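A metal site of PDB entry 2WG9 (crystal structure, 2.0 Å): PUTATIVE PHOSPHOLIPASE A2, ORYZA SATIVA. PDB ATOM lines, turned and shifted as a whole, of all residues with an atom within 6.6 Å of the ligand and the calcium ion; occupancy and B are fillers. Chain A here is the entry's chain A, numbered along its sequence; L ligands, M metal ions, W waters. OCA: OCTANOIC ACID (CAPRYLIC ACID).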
ATOM      1  N   ILE A  30      -0.179  -1.020  34.805  1.00  0.00           N
ATOM      2  CA  ILE A  30       0.781  -0.323  35.659  1.00  0.00           C
ATOM      3  C   ILE A  30       1.658   0.611  34.821  1.00  0.00           C
ATOM      4  O   ILE A  30       2.614   0.170  34.175  1.00  0.00           O
ATOM      5  CB  ILE A  30       1.634  -1.299  36.501  1.00  0.00           C
ATOM      6  CG1 ILE A  30       0.739  -2.156  37.407  1.00  0.00           C
ATOM      7  CG2 ILE A  30       2.684  -0.539  37.327  1.00  0.00           C
ATOM      8  CD1 ILE A  30       1.399  -3.413  37.964  1.00  0.00           C
ATOM      9  N   ALA A  31       1.325   1.903  34.850  1.00  0.00           N
ATOM     10  CA  ALA A  31       1.903   2.909  33.959  1.00  0.00           C
ATOM     11  C   ALA A  31       3.436   2.941  33.899  1.00  0.00           C
ATOM     12  O   ALA A  31       3.995   2.941  32.799  1.00  0.00           O
ATOM     13  CB  ALA A  31       1.330   4.305  34.283  1.00  0.00           C
ATOM     14  N   PRO A  32       4.126   2.973  35.066  1.00  0.00           N
ATOM     15  CA  PRO A  32       5.601   3.023  35.000  1.00  0.00           C
ATOM     16  C   PRO A  32       6.268   1.762  34.459  1.00  0.00           C
ATOM     17  O   PRO A  32       7.421   1.829  34.036  1.00  0.00           O
ATOM     18  CB  PRO A  32       6.019   3.244  36.471  1.00  0.00           C
ATOM     19  CG  PRO A  32       4.757   3.658  37.186  1.00  0.00           C
ATOM     20  CD  PRO A  32       3.653   2.971  36.461  1.00  0.00           C
ATOM     21  N   LEU A  34       4.467  -0.588  32.268  1.00  0.00           N
ATOM     22  CA  LEU A  34       3.774  -1.018  31.055  1.00  0.00           C
ATOM     23  C   LEU A  34       4.743  -1.277  29.903  1.00  0.00           C
ATOM     24  O   LEU A  34       5.611  -0.434  29.615  1.00  0.00           O
ATOM     25  CB  LEU A  34       2.737   0.052  30.665  1.00  0.00           C
ATOM     26  CG  LEU A  34       1.605  -0.248  29.690  1.00  0.00           C
ATOM     27  CD1 LEU A  34       0.396   0.623  30.031  1.00  0.00           C
ATOM     28  CD2 LEU A  34       2.018  -0.024  28.241  1.00  0.00           C
ATOM     29  N   LYS A  38       5.894  -3.264  20.521  1.00  0.00           N
ATOM     30  CA  LYS A  38       7.331  -3.027  20.457  1.00  0.00           C
ATOM     31  C   LYS A  38       7.679  -1.612  20.931  1.00  0.00           C
ATOM     32  O   LYS A  38       8.857  -1.306  21.168  1.00  0.00           O
ATOM     33  CB  LYS A  38       7.866  -3.224  19.025  1.00  0.00           C
ATOM     34  CG  LYS A  38       7.804  -4.648  18.487  1.00  0.00           C
ATOM     35  CD  LYS A  38       8.043  -4.662  16.974  1.00  0.00           C
ATOM     36  CE  LYS A  38       7.776  -6.015  16.341  1.00  0.00           C
ATOM     37  NZ  LYS A  38       8.036  -5.998  14.855  1.00  0.00           N
ATOM     38  N   TYR A  39       6.663  -0.752  21.071  1.00  0.00           N
ATOM     39  CA  TYR A  39       6.879   0.694  21.276  1.00  0.00           C
ATOM     40  C   TYR A  39       6.211   1.333  22.513  1.00  0.00           C
ATOM     41  O   TYR A  39       6.720   2.334  23.016  1.00  0.00           O
ATOM     42  CB  TYR A  39       6.443   1.481  20.014  1.00  0.00           C
ATOM     43  CG  TYR A  39       7.287   1.198  18.783  1.00  0.00           C
ATOM     44  CD1 TYR A  39       6.909   0.223  17.856  1.00  0.00           C
ATOM     45  CD2 TYR A  39       8.459   1.916  18.549  1.00  0.00           C
ATOM     46  CE1 TYR A  39       7.694  -0.031  16.722  1.00  0.00           C
ATOM     47  CE2 TYR A  39       9.255   1.654  17.419  1.00  0.00           C
ATOM     48  CZ  TYR A  39       8.868   0.681  16.519  1.00  0.00           C
ATOM     49  OH  TYR A  39       9.654   0.437  15.399  1.00  0.00           O
ATOM     50  N   CYS A  40       5.098   0.798  22.997  1.00  0.00           N
ATOM     51  CA  CYS A  40       4.367   1.437  24.099  1.00  0.00           C
ATOM     52  C   CYS A  40       4.980   1.127  25.466  1.00  0.00           C
ATOM     53  O   CYS A  40       4.997  -0.019  25.920  1.00  0.00           O
ATOM     54  CB  CYS A  40       2.881   1.060  24.093  1.00  0.00           C
ATOM     55  SG  CYS A  40       1.912   1.594  22.658  1.00  0.00           S
ATOM     56  N   GLY A  41       5.493   2.168  26.116  1.00  0.00           N
ATOM     57  CA  GLY A  41       6.095   2.032  27.430  1.00  0.00           C
ATOM     58  C   GLY A  41       7.188   3.068  27.629  1.00  0.00           C
ATOM     59  O   GLY A  41       7.782   3.553  26.674  1.00  0.00           O
ATOM     60  N   ILE A  42       7.448   3.392  28.890  1.00  0.00           N
ATOM     61  CA  ILE A  42       8.471   4.371  29.237  1.00  0.00           C
ATOM     62  C   ILE A  42       9.848   3.741  29.062  1.00  0.00           C
ATOM     63  O   ILE A  42      10.075   2.620  29.512  1.00  0.00           O
ATOM     64  CB  ILE A  42       8.250   4.912  30.681  1.00  0.00           C
ATOM     65  CG1 ILE A  42       6.872   5.576  30.790  1.00  0.00           C
ATOM     66  CG2 ILE A  42       9.377   5.884  31.080  1.00  0.00           C
ATOM     67  CD1 ILE A  42       6.369   5.789  32.217  1.00  0.00           C
ATOM     68  N   LEU A  43      10.749   4.450  28.401  1.00  0.00           N
ATOM     69  CA  LEU A  43      12.101   3.928  28.108  1.00  0.00           C
ATOM     70  C   LEU A  43      12.024   2.506  27.542  1.00  0.00           C
ATOM     71  O   LEU A  43      12.709   1.590  27.994  1.00  0.00           O
ATOM     72  CB  LEU A  43      13.009   4.029  29.352  1.00  0.00           C
ATOM     73  CG  LEU A  43      13.168   5.421  29.980  1.00  0.00           C
ATOM     74  CD1 LEU A  43      13.813   5.347  31.347  1.00  0.00           C
ATOM     75  CD2 LEU A  43      13.927   6.387  29.081  1.00  0.00           C
ATOM     76  N   TYR A  44      11.133   2.344  26.560  1.00  0.00           N
ATOM     77  CA  TYR A  44      10.910   1.077  25.888  1.00  0.00           C
ATOM     78  C   TYR A  44      10.487   1.398  24.450  1.00  0.00           C
ATOM     79  O   TYR A  44       9.471   2.071  24.241  1.00  0.00           O
ATOM     80  CB  TYR A  44       9.815   0.265  26.597  1.00  0.00           C
ATOM     81  CG  TYR A  44       9.404  -0.954  25.815  1.00  0.00           C
ATOM     82  CD1 TYR A  44      10.257  -2.064  25.737  1.00  0.00           C
ATOM     83  CD2 TYR A  44       8.187  -1.011  25.136  1.00  0.00           C
ATOM     84  CE1 TYR A  44       9.899  -3.192  25.016  1.00  0.00           C
ATOM     85  CE2 TYR A  44       7.825  -2.135  24.406  1.00  0.00           C
ATOM     86  CZ  TYR A  44       8.694  -3.223  24.354  1.00  0.00           C
ATOM     87  OH  TYR A  44       8.354  -4.340  23.630  1.00  0.00           O
ATOM     88  N   SER A  45      11.258   0.935  23.478  1.00  0.00           N
ATOM     89  CA  SER A  45      10.981   1.271  22.075  1.00  0.00           C
ATOM     90  C   SER A  45      11.501   0.206  21.120  1.00  0.00           C
ATOM     91  O   SER A  45      12.362  -0.611  21.472  1.00  0.00           O
ATOM     92  CB  SER A  45      11.583   2.642  21.723  1.00  0.00           C
ATOM     93  OG  SER A  45      10.897   3.228  20.615  1.00  0.00           O
ATOM     94  N   GLY A  46      10.969   0.205  19.900  1.00  0.00           N
ATOM     95  CA  GLY A  46      11.291  -0.800  18.899  1.00  0.00           C
ATOM     96  C   GLY A  46      12.586  -0.472  18.179  1.00  0.00           C
ATOM     97  O   GLY A  46      12.976   0.685  18.064  1.00  0.00           O
ATOM     98  N   CYS A  59       0.774   4.190  17.240  1.00  0.00           N
ATOM     99  CA  CYS A  59       0.701   5.496  17.902  1.00  0.00           C
ATOM    100  C   CYS A  59       1.953   5.753  18.744  1.00  0.00           C
ATOM    101  O   CYS A  59       2.542   6.835  18.692  1.00  0.00           O
ATOM    102  CB  CYS A  59      -0.543   5.600  18.809  1.00  0.00           C
ATOM    103  SG  CYS A  59      -2.115   5.548  17.937  1.00  0.00           S
ATOM    104  N   CYS A  60       2.355   4.749  19.513  1.00  0.00           N
ATOM    105  CA  CYS A  60       3.563   4.843  20.342  1.00  0.00           C
ATOM    106  C   CYS A  60       4.847   4.968  19.529  1.00  0.00           C
ATOM    107  O   CYS A  60       5.758   5.728  19.899  1.00  0.00           O
ATOM    108  CB  CYS A  60       3.656   3.640  21.274  1.00  0.00           C
ATOM    109  SG  CYS A  60       2.305   3.572  22.465  1.00  0.00           S
ATOM    110  N   MET A  61       4.931   4.220  18.422  1.00  0.00           N
ATOM    111  CA  MET A  61       6.076   4.333  17.516  1.00  0.00           C
ATOM    112  C   MET A  61       6.294   5.769  17.059  1.00  0.00           C
ATOM    113  O   MET A  61       7.419   6.282  17.133  1.00  0.00           O
ATOM    114  CB  MET A  61       5.902   3.427  16.291  1.00  0.00           C
ATOM    115  CG  MET A  61       7.032   3.554  15.272  1.00  0.00           C
ATOM    116  SD  MET A  61       6.670   2.631  13.780  1.00  0.00           S
ATOM    117  CE  MET A  61       8.283   2.671  12.971  1.00  0.00           C
ATOM    118  N   VAL A  62       5.235   6.421  16.589  1.00  0.00           N
ATOM    119  CA  VAL A  62       5.320   7.834  16.178  1.00  0.00           C
ATOM    120  C   VAL A  62       5.763   8.708  17.336  1.00  0.00           C
ATOM    121  O   VAL A  62       6.614   9.593  17.180  1.00  0.00           O
ATOM    122  CB  VAL A  62       3.978   8.355  15.608  1.00  0.00           C
ATOM    123  CG1 VAL A  62       4.008   9.875  15.423  1.00  0.00           C
ATOM    124  CG2 VAL A  62       3.654   7.691  14.288  1.00  0.00           C
ATOM    125  N   HIS A  63       5.184   8.466  18.509  1.00  0.00           N
ATOM    126  CA  HIS A  63       5.501   9.277  19.697  1.00  0.00           C
ATOM    127  C   HIS A  63       6.980   9.176  20.086  1.00  0.00           C
ATOM    128  O   HIS A  63       7.618  10.191  20.361  1.00  0.00           O
ATOM    129  CB  HIS A  63       4.617   8.892  20.885  1.00  0.00           C
ATOM    130  CG  HIS A  63       4.947   9.647  22.136  1.00  0.00           C
ATOM    131  ND1 HIS A  63       5.884   9.207  23.037  1.00  0.00           N
ATOM    132  CD2 HIS A  63       4.453  10.804  22.637  1.00  0.00           C
ATOM    133  CE1 HIS A  63       5.972  10.070  24.040  1.00  0.00           C
ATOM    134  NE2 HIS A  63       5.113  11.040  23.823  1.00  0.00           N
ATOM    135  N   ASP A  64       7.512   7.957  20.119  1.00  0.00           N
ATOM    136  CA  ASP A  64       8.901   7.731  20.536  1.00  0.00           C
ATOM    137  C   ASP A  64       9.880   8.467  19.636  1.00  0.00           C
ATOM    138  O   ASP A  64      10.823   9.104  20.106  1.00  0.00           O
ATOM    139  CB  ASP A  64       9.206   6.229  20.574  1.00  0.00           C
ATOM    140  CG  ASP A  64       8.482   5.528  21.703  1.00  0.00           C
ATOM    141  OD1 ASP A  64       7.742   6.198  22.452  1.00  0.00           O
ATOM    142  OD2 ASP A  64       8.634   4.293  21.845  1.00  0.00           O
ATOM    143  N   ASN A  80       2.923  14.868  22.365  1.00  0.00           N
ATOM    144  CA  ASN A  80       1.922  14.342  23.294  1.00  0.00           C
ATOM    145  C   ASN A  80       0.470  14.532  22.828  1.00  0.00           C
ATOM    146  O   ASN A  80      -0.336  13.608  22.944  1.00  0.00           O
ATOM    147  CB  ASN A  80       2.171  14.901  24.690  1.00  0.00           C
ATOM    148  CG  ASN A  80       3.420  14.313  25.333  1.00  0.00           C
ATOM    149  OD1 ASN A  80       3.686  13.118  25.217  1.00  0.00           O
ATOM    150  ND2 ASN A  80       4.205  15.160  25.988  1.00  0.00           N
ATOM    151  N   LEU A  83      -0.244  12.075  20.128  1.00  0.00           N
ATOM    152  CA  LEU A  83      -0.448  10.747  20.720  1.00  0.00           C
ATOM    153  C   LEU A  83      -1.897  10.573  21.202  1.00  0.00           C
ATOM    154  O   LEU A  83      -2.531   9.557  20.914  1.00  0.00           O
ATOM    155  CB  LEU A  83       0.560  10.460  21.855  1.00  0.00           C
ATOM    156  CG  LEU A  83       0.507   9.076  22.522  1.00  0.00           C
ATOM    157  CD1 LEU A  83       0.530   7.928  21.500  1.00  0.00           C
ATOM    158  CD2 LEU A  83       1.627   8.865  23.514  1.00  0.00           C
ATOM    159  N   THR A 105      -5.535  -0.567  28.115  1.00  0.00           N
ATOM    160  CA  THR A 105      -4.147  -0.098  28.053  1.00  0.00           C
ATOM    161  C   THR A 105      -4.074   1.310  27.465  1.00  0.00           C
ATOM    162  O   THR A 105      -3.325   2.154  27.965  1.00  0.00           O
ATOM    163  CB  THR A 105      -3.244  -1.073  27.261  1.00  0.00           C
ATOM    164  OG1 THR A 105      -3.190  -2.337  27.937  1.00  0.00           O
ATOM    165  CG2 THR A 105      -1.821  -0.533  27.113  1.00  0.00           C
ATOM    166  N   VAL A 108      -4.931   3.853  30.093  1.00  0.00           N
ATOM    167  CA  VAL A 108      -3.817   4.035  31.030  1.00  0.00           C
ATOM    168  C   VAL A 108      -2.748   4.974  30.432  1.00  0.00           C
ATOM    169  O   VAL A 108      -2.278   5.910  31.079  1.00  0.00           O
ATOM    170  CB  VAL A 108      -3.213   2.681  31.503  1.00  0.00           C
ATOM    171  CG1 VAL A 108      -1.982   2.887  32.389  1.00  0.00           C
ATOM    172  CG2 VAL A 108      -4.265   1.847  32.246  1.00  0.00           C
ATOM    173  N   ILE A 109      -2.394   4.735  29.167  1.00  0.00           N
ATOM    174  CA  ILE A 109      -1.457   5.610  28.454  1.00  0.00           C
ATOM    175  C   ILE A 109      -2.049   7.014  28.365  1.00  0.00           C
ATOM    176  O   ILE A 109      -1.358   8.003  28.646  1.00  0.00           O
ATOM    177  CB  ILE A 109      -1.117   5.068  27.038  1.00  0.00           C
ATOM    178  CG1 ILE A 109      -0.402   3.707  27.159  1.00  0.00           C
ATOM    179  CG2 ILE A 109      -0.266   6.075  26.257  1.00  0.00           C
ATOM    180  CD1 ILE A 109      -0.413   2.852  25.887  1.00  0.00           C
ATOM    181  N   ARG A 110      -3.327   7.096  27.980  1.00  0.00           N
ATOM    182  CA  ARG A 110      -4.006   8.376  27.806  1.00  0.00           C
ATOM    183  C   ARG A 110      -3.949   9.239  29.054  1.00  0.00           C
ATOM    184  O   ARG A 110      -3.656  10.423  28.970  1.00  0.00           O
ATOM    185  CB  ARG A 110      -5.462   8.183  27.368  1.00  0.00           C
ATOM    186  CG  ARG A 110      -5.943   9.319  26.495  1.00  0.00           C
ATOM    187  CD  ARG A 110      -7.468   9.535  26.499  1.00  0.00           C
ATOM    188  NE  ARG A 110      -7.835  10.480  25.440  1.00  0.00           N
ATOM    189  CZ  ARG A 110      -7.752  11.813  25.535  1.00  0.00           C
ATOM    190  NH1 ARG A 110      -7.346  12.384  26.661  1.00  0.00           N
ATOM    191  NH2 ARG A 110      -8.095  12.576  24.513  1.00  0.00           N
ATOM    192  N   VAL A 112      -1.731   9.319  31.531  1.00  0.00           N
ATOM    193  CA  VAL A 112      -0.366   9.809  31.707  1.00  0.00           C
ATOM    194  C   VAL A 112      -0.019  10.919  30.707  1.00  0.00           C
ATOM    195  O   VAL A 112       0.597  11.936  31.080  1.00  0.00           O
ATOM    196  CB  VAL A 112       0.659   8.646  31.575  1.00  0.00           C
ATOM    197  CG1 VAL A 112       2.106   9.153  31.552  1.00  0.00           C
ATOM    198  CG2 VAL A 112       0.467   7.642  32.708  1.00  0.00           C
ATOM    199  N   ILE A 113      -0.410  10.736  29.452  1.00  0.00           N
ATOM    200  CA  ILE A 113      -0.093  11.701  28.398  1.00  0.00           C
ATOM    201  C   ILE A 113      -0.867  13.017  28.548  1.00  0.00           C
ATOM    202  O   ILE A 113      -0.328  14.093  28.253  1.00  0.00           O
ATOM    203  CB  ILE A 113      -0.241  11.074  26.977  1.00  0.00           C
ATOM    204  CG1 ILE A 113       0.733   9.891  26.799  1.00  0.00           C
ATOM    205  CG2 ILE A 113       0.012  12.118  25.861  1.00  0.00           C
ATOM    206  CD1 ILE A 113       2.234  10.227  27.041  1.00  0.00           C
HETATM  207  C1  OCA L   1       5.017   5.606  24.138  1.00  0.00           C
HETATM  208  C2  OCA L   1       3.727   5.844  24.931  1.00  0.00           C
HETATM  209  C3  OCA L   1       3.872   6.987  25.930  1.00  0.00           C
HETATM  210  C4  OCA L   1       4.729   6.599  27.143  1.00  0.00           C
HETATM  211  C5  OCA L   1       4.094   5.480  27.990  1.00  0.00           C
HETATM  212  C6  OCA L   1       3.127   6.048  29.032  1.00  0.00           C
HETATM  213  C7  OCA L   1       3.070   5.145  30.269  1.00  0.00           C
HETATM  214  C8  OCA L   1       1.719   4.426  30.350  1.00  0.00           C
HETATM  215  O1  OCA L   1       5.816   4.759  24.577  1.00  0.00           O
HETATM  216  O2  OCA L   1       5.162   6.284  23.101  1.00  0.00           O
HETATM  217 CA    CA M   1       8.029   3.769  24.150  1.00  0.00          CA
HETATM  218  O   HOH W   1       9.828   5.114  25.023  1.00  0.00           O
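Water W1 lies within hydrogen-bond range of the backbone NH of Tyr 44 (3.4 Å) and the side-chain carboxylate of Asp 64 (3.5 Å).
A ring nitrogen (ND1) of His 63 sits at hydrogen-bond distance from an oxygen (O2) of the ligand (3.0 Å). N of Gly 41 lies close to O1 of the ligand, at 3.0 Å.
OD1 of Asn 80 sits at hydrogen-bond distance from NE2 of His 63, 2.9 Å away. The side-chain sulfur (SG) of Cys 60 is disulfide-bonded to the side-chain sulfur (SG) of Cys 40 (2.0 Å). OG of Ser 45 sits close to OD2 of Asp 64 (2.8 Å).
An oxygen (O2) of the ligand sits close to the backbone carbonyl oxygen of Cys 60, at 3.3 Å. Residues that only touch the ligand: Ala 31, Cys 40, Leu 83, Ile 113, Ile 42 and Ile 109. Of the 27 residues printed, 11 come within 4 Å of the ligand.
O of Tyr 44 binds the calcium ion (2.2 Å). O of Tyr 39 binds the calcium ion. Water W1 binds the calcium ion, 2.4 Å away. OD2 of Asp 64 binds the calcium ion, 2.4 Å away. The calcium ion is bound by an oxygen (O1) of the ligand. O of Gly 41 binds the calcium ion (2.5 Å). The calcium ion has six donor atoms within binding distance. Slightly farther from the calcium ion lies OD1 of Asp 64 (3.0 Å).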
